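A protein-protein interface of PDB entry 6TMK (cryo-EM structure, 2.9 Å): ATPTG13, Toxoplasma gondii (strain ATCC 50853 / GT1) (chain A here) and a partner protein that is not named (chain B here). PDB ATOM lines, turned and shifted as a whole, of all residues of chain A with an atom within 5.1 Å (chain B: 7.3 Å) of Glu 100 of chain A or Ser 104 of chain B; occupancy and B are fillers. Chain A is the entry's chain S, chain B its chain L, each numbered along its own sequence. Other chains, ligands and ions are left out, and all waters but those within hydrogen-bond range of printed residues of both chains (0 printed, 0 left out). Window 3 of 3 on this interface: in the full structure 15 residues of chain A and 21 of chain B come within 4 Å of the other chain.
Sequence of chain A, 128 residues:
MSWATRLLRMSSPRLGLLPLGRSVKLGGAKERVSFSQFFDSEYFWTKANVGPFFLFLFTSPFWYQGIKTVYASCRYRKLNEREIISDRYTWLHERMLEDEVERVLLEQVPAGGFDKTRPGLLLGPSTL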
ATOM      1  N   MET A  96     -24.981 -23.469  26.934  1.00  0.00           N
ATOM      2  CA  MET A  96     -24.118 -23.725  25.788  1.00  0.00           C
ATOM      3  C   MET A  96     -22.908 -22.800  25.794  1.00  0.00           C
ATOM      4  O   MET A  96     -21.795 -23.215  25.443  1.00  0.00           O
ATOM      5  CB  MET A  96     -24.918 -23.572  24.502  1.00  0.00           C
ATOM      6  CG  MET A  96     -25.914 -24.689  24.280  1.00  0.00           C
ATOM      7  SD  MET A  96     -27.092 -24.359  22.969  1.00  0.00           S
ATOM      8  CE  MET A  96     -26.137 -24.875  21.558  1.00  0.00           C
ATOM      9  N   LEU A  97     -23.101 -21.545  26.199  1.00  0.00           N
ATOM     10  CA  LEU A  97     -21.957 -20.650  26.342  1.00  0.00           C
ATOM     11  C   LEU A  97     -20.985 -21.162  27.398  1.00  0.00           C
ATOM     12  O   LEU A  97     -19.760 -21.137  27.203  1.00  0.00           O
ATOM     13  CB  LEU A  97     -22.428 -19.246  26.696  1.00  0.00           C
ATOM     14  CG  LEU A  97     -23.258 -18.524  25.641  1.00  0.00           C
ATOM     15  CD1 LEU A  97     -23.708 -17.190  26.161  1.00  0.00           C
ATOM     16  CD2 LEU A  97     -22.490 -18.358  24.366  1.00  0.00           C
ATOM     17  N   GLU A  98     -21.514 -21.629  28.529  1.00  0.00           N
ATOM     18  CA  GLU A  98     -20.661 -22.221  29.554  1.00  0.00           C
ATOM     19  C   GLU A  98     -19.886 -23.414  29.008  1.00  0.00           C
ATOM     20  O   GLU A  98     -18.705 -23.598  29.327  1.00  0.00           O
ATOM     21  CB  GLU A  98     -21.509 -22.652  30.743  1.00  0.00           C
ATOM     22  CG  GLU A  98     -21.968 -21.530  31.627  1.00  0.00           C
ATOM     23  CD  GLU A  98     -22.912 -22.008  32.708  1.00  0.00           C
ATOM     24  OE1 GLU A  98     -23.114 -23.234  32.820  1.00  0.00           O
ATOM     25  OE2 GLU A  98     -23.461 -21.158  33.440  1.00  0.00           O
ATOM     26  N   ASP A  99     -20.538 -24.239  28.191  1.00  0.00           N
ATOM     27  CA  ASP A  99     -19.866 -25.402  27.625  1.00  0.00           C
ATOM     28  C   ASP A  99     -18.742 -24.985  26.688  1.00  0.00           C
ATOM     29  O   ASP A  99     -17.678 -25.612  26.667  1.00  0.00           O
ATOM     30  CB  ASP A  99     -20.872 -26.285  26.897  1.00  0.00           C
ATOM     31  CG  ASP A  99     -21.875 -26.923  27.837  1.00  0.00           C
ATOM     32  OD1 ASP A  99     -21.598 -26.980  29.054  1.00  0.00           O
ATOM     33  OD2 ASP A  99     -22.940 -27.370  27.361  1.00  0.00           O
ATOM     34  N   GLU A 100     -18.960 -23.933  25.902  1.00  0.00           N
ATOM     35  CA  GLU A 100     -17.896 -23.424  25.040  1.00  0.00           C
ATOM     36  C   GLU A 100     -16.707 -22.954  25.868  1.00  0.00           C
ATOM     37  O   GLU A 100     -15.544 -23.247  25.546  1.00  0.00           O
ATOM     38  CB  GLU A 100     -18.427 -22.284  24.177  1.00  0.00           C
ATOM     39  CG  GLU A 100     -17.421 -21.745  23.190  1.00  0.00           C
ATOM     40  CD  GLU A 100     -18.014 -20.693  22.275  1.00  0.00           C
ATOM     41  OE1 GLU A 100     -17.241 -19.995  21.584  1.00  0.00           O
ATOM     42  OE2 GLU A 100     -19.256 -20.564  22.246  1.00  0.00           O
ATOM     43  N   VAL A 101     -16.982 -22.212  26.938  1.00  0.00           N
ATOM     44  CA  VAL A 101     -15.905 -21.739  27.803  1.00  0.00           C
ATOM     45  C   VAL A 101     -15.128 -22.915  28.379  1.00  0.00           C
ATOM     46  O   VAL A 101     -13.892 -22.899  28.423  1.00  0.00           O
ATOM     47  CB  VAL A 101     -16.473 -20.840  28.914  1.00  0.00           C
ATOM     48  CG1 VAL A 101     -15.415 -20.546  29.952  1.00  0.00           C
ATOM     49  CG2 VAL A 101     -17.004 -19.562  28.325  1.00  0.00           C
ATOM     50  N   GLU A 102     -15.835 -23.944  28.845  1.00  0.00           N
ATOM     51  CA  GLU A 102     -15.158 -25.114  29.394  1.00  0.00           C
ATOM     52  C   GLU A 102     -14.316 -25.818  28.337  1.00  0.00           C
ATOM     53  O   GLU A 102     -13.211 -26.294  28.625  1.00  0.00           O
ATOM     54  CB  GLU A 102     -16.181 -26.076  29.985  1.00  0.00           C
ATOM     55  CG  GLU A 102     -15.569 -27.252  30.719  1.00  0.00           C
ATOM     56  CD  GLU A 102     -16.566 -27.986  31.591  1.00  0.00           C
ATOM     57  OE1 GLU A 102     -16.564 -29.235  31.571  1.00  0.00           O
ATOM     58  OE2 GLU A 102     -17.349 -27.318  32.300  1.00  0.00           O
ATOM     59  N   ARG A 103     -14.832 -25.916  27.111  1.00  0.00           N
ATOM     60  CA  ARG A 103     -14.071 -26.552  26.043  1.00  0.00           C
ATOM     61  C   ARG A 103     -12.783 -25.798  25.766  1.00  0.00           C
ATOM     62  O   ARG A 103     -11.749 -26.408  25.468  1.00  0.00           O
ATOM     63  CB  ARG A 103     -14.910 -26.648  24.774  1.00  0.00           C
ATOM     64  CG  ARG A 103     -14.261 -27.494  23.696  1.00  0.00           C
ATOM     65  CD  ARG A 103     -15.171 -27.763  22.508  1.00  0.00           C
ATOM     66  NE  ARG A 103     -16.436 -28.382  22.898  1.00  0.00           N
ATOM     67  CZ  ARG A 103     -17.592 -27.737  23.021  1.00  0.00           C
ATOM     68  NH1 ARG A 103     -17.675 -26.434  22.790  1.00  0.00           N
ATOM     69  NH2 ARG A 103     -18.677 -28.402  23.384  1.00  0.00           N
ATOM     70  N   VAL A 104     -12.821 -24.470  25.853  1.00  0.00           N
ATOM     71  CA  VAL A 104     -11.593 -23.705  25.669  1.00  0.00           C
ATOM     72  C   VAL A 104     -10.659 -23.884  26.860  1.00  0.00           C
ATOM     73  O   VAL A 104      -9.435 -23.944  26.701  1.00  0.00           O
ATOM     74  CB  VAL A 104     -11.915 -22.222  25.426  1.00  0.00           C
ATOM     75  CG1 VAL A 104     -10.699 -21.372  25.688  1.00  0.00           C
ATOM     76  CG2 VAL A 104     -12.383 -22.023  24.008  1.00  0.00           C
ATOM     77  N   LEU A 105     -11.214 -23.965  28.070  1.00  0.00           N
ATOM     78  CA  LEU A 105     -10.373 -24.074  29.258  1.00  0.00           C
ATOM     79  C   LEU A 105      -9.630 -25.400  29.298  1.00  0.00           C
ATOM     80  O   LEU A 105      -8.478 -25.459  29.738  1.00  0.00           O
ATOM     81  CB  LEU A 105     -11.211 -23.922  30.522  1.00  0.00           C
ATOM     82  CG  LEU A 105     -11.734 -22.539  30.891  1.00  0.00           C
ATOM     83  CD1 LEU A 105     -12.570 -22.645  32.135  1.00  0.00           C
ATOM     84  CD2 LEU A 105     -10.606 -21.566  31.107  1.00  0.00           C
ATOM     85  N   GLU B 100      -9.702 -15.565  25.225  1.00  0.00           N
ATOM     86  CA  GLU B 100      -9.065 -16.016  24.001  1.00  0.00           C
ATOM     87  C   GLU B 100      -9.809 -15.483  22.785  1.00  0.00           C
ATOM     88  O   GLU B 100     -11.020 -15.252  22.823  1.00  0.00           O
ATOM     89  CB  GLU B 100      -9.019 -17.542  23.956  1.00  0.00           C
ATOM     90  CG  GLU B 100      -8.013 -18.144  24.908  1.00  0.00           C
ATOM     91  CD  GLU B 100      -8.521 -18.187  26.331  1.00  0.00           C
ATOM     92  OE1 GLU B 100      -9.506 -17.482  26.627  1.00  0.00           O
ATOM     93  OE2 GLU B 100      -7.937 -18.922  27.154  1.00  0.00           O
ATOM     94  N   ASP B 101      -9.064 -15.290  21.696  1.00  0.00           N
ATOM     95  CA  ASP B 101      -9.666 -14.817  20.458  1.00  0.00           C
ATOM     96  C   ASP B 101     -10.499 -15.893  19.780  1.00  0.00           C
ATOM     97  O   ASP B 101     -11.352 -15.569  18.948  1.00  0.00           O
ATOM     98  CB  ASP B 101      -8.572 -14.332  19.508  1.00  0.00           C
ATOM     99  CG  ASP B 101      -7.628 -13.345  20.162  1.00  0.00           C
ATOM    100  OD1 ASP B 101      -6.399 -13.548  20.071  1.00  0.00           O
ATOM    101  OD2 ASP B 101      -8.114 -12.368  20.768  1.00  0.00           O
ATOM    102  N   LYS B 102     -10.269 -17.161  20.118  1.00  0.00           N
ATOM    103  CA  LYS B 102     -11.096 -18.237  19.589  1.00  0.00           C
ATOM    104  C   LYS B 102     -12.560 -18.045  19.959  1.00  0.00           C
ATOM    105  O   LYS B 102     -13.456 -18.362  19.169  1.00  0.00           O
ATOM    106  CB  LYS B 102     -10.584 -19.578  20.104  1.00  0.00           C
ATOM    107  CG  LYS B 102     -11.201 -20.778  19.427  1.00  0.00           C
ATOM    108  CD  LYS B 102     -10.753 -22.067  20.085  1.00  0.00           C
ATOM    109  CE  LYS B 102      -9.358 -22.463  19.637  1.00  0.00           C
ATOM    110  NZ  LYS B 102      -9.328 -22.914  18.218  1.00  0.00           N
ATOM    111  N   LEU B 103     -12.821 -17.532  21.157  1.00  0.00           N
ATOM    112  CA  LEU B 103     -14.181 -17.455  21.661  1.00  0.00           C
ATOM    113  C   LEU B 103     -14.982 -16.375  20.944  1.00  0.00           C
ATOM    114  O   LEU B 103     -14.437 -15.389  20.442  1.00  0.00           O
ATOM    115  CB  LEU B 103     -14.178 -17.168  23.159  1.00  0.00           C
ATOM    116  CG  LEU B 103     -13.720 -18.281  24.090  1.00  0.00           C
ATOM    117  CD1 LEU B 103     -13.591 -17.747  25.491  1.00  0.00           C
ATOM    118  CD2 LEU B 103     -14.688 -19.427  24.060  1.00  0.00           C
ATOM    119  N   SER B 104     -16.294 -16.575  20.910  1.00  0.00           N
ATOM    120  CA  SER B 104     -17.228 -15.539  20.514  1.00  0.00           C
ATOM    121  C   SER B 104     -17.418 -14.536  21.645  1.00  0.00           C
ATOM    122  O   SER B 104     -17.176 -14.831  22.816  1.00  0.00           O
ATOM    123  CB  SER B 104     -18.573 -16.146  20.128  1.00  0.00           C
ATOM    124  OG  SER B 104     -19.273 -16.598  21.269  1.00  0.00           O
ATOM    125  N   VAL B 105     -17.860 -13.335  21.275  1.00  0.00           N
ATOM    126  CA  VAL B 105     -17.931 -12.238  22.236  1.00  0.00           C
ATOM    127  C   VAL B 105     -18.860 -12.586  23.391  1.00  0.00           C
ATOM    128  O   VAL B 105     -18.615 -12.201  24.541  1.00  0.00           O
ATOM    129  CB  VAL B 105     -18.370 -10.949  21.522  1.00  0.00           C
ATOM    130  CG1 VAL B 105     -18.694  -9.871  22.529  1.00  0.00           C
ATOM    131  CG2 VAL B 105     -17.290 -10.488  20.570  1.00  0.00           C
ATOM    132  N   ASP B 106     -19.932 -13.325  23.112  1.00  0.00           N
ATOM    133  CA  ASP B 106     -20.828 -13.752  24.182  1.00  0.00           C
ATOM    134  C   ASP B 106     -20.111 -14.666  25.166  1.00  0.00           C
ATOM    135  O   ASP B 106     -20.258 -14.523  26.386  1.00  0.00           O
ATOM    136  CB  ASP B 106     -22.045 -14.454  23.587  1.00  0.00           C
ATOM    137  CG  ASP B 106     -23.013 -13.492  22.937  1.00  0.00           C
ATOM    138  OD1 ASP B 106     -22.800 -12.266  23.048  1.00  0.00           O
ATOM    139  OD2 ASP B 106     -23.986 -13.963  22.312  1.00  0.00           O
ATOM    140  N   ALA B 107     -19.317 -15.603  24.653  1.00  0.00           N
ATOM    141  CA  ALA B 107     -18.591 -16.509  25.526  1.00  0.00           C
ATOM    142  C   ALA B 107     -17.486 -15.786  26.280  1.00  0.00           C
ATOM    143  O   ALA B 107     -17.165 -16.157  27.411  1.00  0.00           O
ATOM    144  CB  ALA B 107     -18.021 -17.661  24.710  1.00  0.00           C
ATOM    145  N   ARG B 108     -16.896 -14.759  25.675  1.00  0.00           N
ATOM    146  CA  ARG B 108     -15.926 -13.934  26.383  1.00  0.00           C
ATOM    147  C   ARG B 108     -16.584 -13.212  27.549  1.00  0.00           C
ATOM    148  O   ARG B 108     -16.037 -13.157  28.657  1.00  0.00           O
ATOM    149  CB  ARG B 108     -15.308 -12.927  25.421  1.00  0.00           C
ATOM    150  CG  ARG B 108     -14.539 -13.535  24.291  1.00  0.00           C
ATOM    151  CD  ARG B 108     -14.030 -12.462  23.370  1.00  0.00           C
ATOM    152  NE  ARG B 108     -13.526 -12.996  22.113  1.00  0.00           N
ATOM    153  CZ  ARG B 108     -13.055 -12.240  21.131  1.00  0.00           C
ATOM    154  NH1 ARG B 108     -13.024 -10.926  21.265  1.00  0.00           N
ATOM    155  NH2 ARG B 108     -12.617 -12.799  20.018  1.00  0.00           N
ATOM    156  N   GLU B 109     -17.752 -12.622  27.301  1.00  0.00           N
ATOM    157  CA  GLU B 109     -18.522 -12.010  28.373  1.00  0.00           C
ATOM    158  C   GLU B 109     -18.808 -13.015  29.480  1.00  0.00           C
ATOM    159  O   GLU B 109     -18.682 -12.699  30.668  1.00  0.00           O
ATOM    160  CB  GLU B 109     -19.819 -11.442  27.809  1.00  0.00           C
ATOM    161  CG  GLU B 109     -20.582 -10.547  28.754  1.00  0.00           C
ATOM    162  CD  GLU B 109     -21.869 -10.029  28.152  1.00  0.00           C
ATOM    163  OE1 GLU B 109     -22.877  -9.947  28.882  1.00  0.00           O
ATOM    164  OE2 GLU B 109     -21.872  -9.708  26.945  1.00  0.00           O
ATOM    165  N   MET B 110     -19.187 -14.237  29.105  1.00  0.00           N
ATOM    166  CA  MET B 110     -19.479 -15.261  30.101  1.00  0.00           C
ATOM    167  C   MET B 110     -18.239 -15.615  30.913  1.00  0.00           C
ATOM    168  O   MET B 110     -18.311 -15.774  32.136  1.00  0.00           O
ATOM    169  CB  MET B 110     -20.044 -16.497  29.410  1.00  0.00           C
ATOM    170  CG  MET B 110     -20.378 -17.651  30.330  1.00  0.00           C
ATOM    171  SD  MET B 110     -21.425 -17.187  31.712  1.00  0.00           S
ATOM    172  CE  MET B 110     -22.998 -17.158  30.879  1.00  0.00           C
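OE1 of Glu 100 of chain A touches CD2 of Leu 103 of chain B, at 3.6 Å.
Glu 100 of chain A touches Ser 104 of chain B (OE1 to N, 3.6 Å).
Glu 100 of chain A touches Ala 107 of chain B.
Ala 107 of chain B touches Val 101 of chain A (O to CG2, 3.5 Å).
Val 104 of chain A touches Glu 100 of chain B.
Val 104 of chain A touches Leu 103 of chain B (CG2 to CD2, 3.5 Å).
Of the printed residues of chain B, Val 101 of chain A touches Ala 107 (3.5 Å).
Of the printed residues of chain B, Val 104 of chain A touches Glu 100 and Leu 103.
Printed residues of chain A within 4 Å of Glu 100 of chain B: Val 104 (3.9 Å).
Ser 104 of chain B touches just one residue of chain A: Glu 100.
Of the printed residues of chain A, Ala 107 of chain B touches Glu 100 and Val 101.
The nearest residue of chain B that does not touch Glu 100 of chain A is Lys 102 of chain B (4.8 Å).
The nearest residue of chain A that does not touch Ser 104 of chain B is Leu 97 of chain A (4.8 Å).
The nearest printed residue of chain A that does not touch Leu 103 of chain B is Val 101 of chain A (4.6 Å).
O of Glu 100 of chain B sits at hydrogen-bond distance from NE of Arg 108 of chain B.
The guanidinium group (NE) of Arg 108 of chain B sits at hydrogen-bond distance from the backbone carbonyl oxygen (O) of Leu 103 of chain B, at 3.1 Å.
Hydrophobic or aromatic side chains of chain A that line the printed part of chain B: Val 101 and Val 104.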
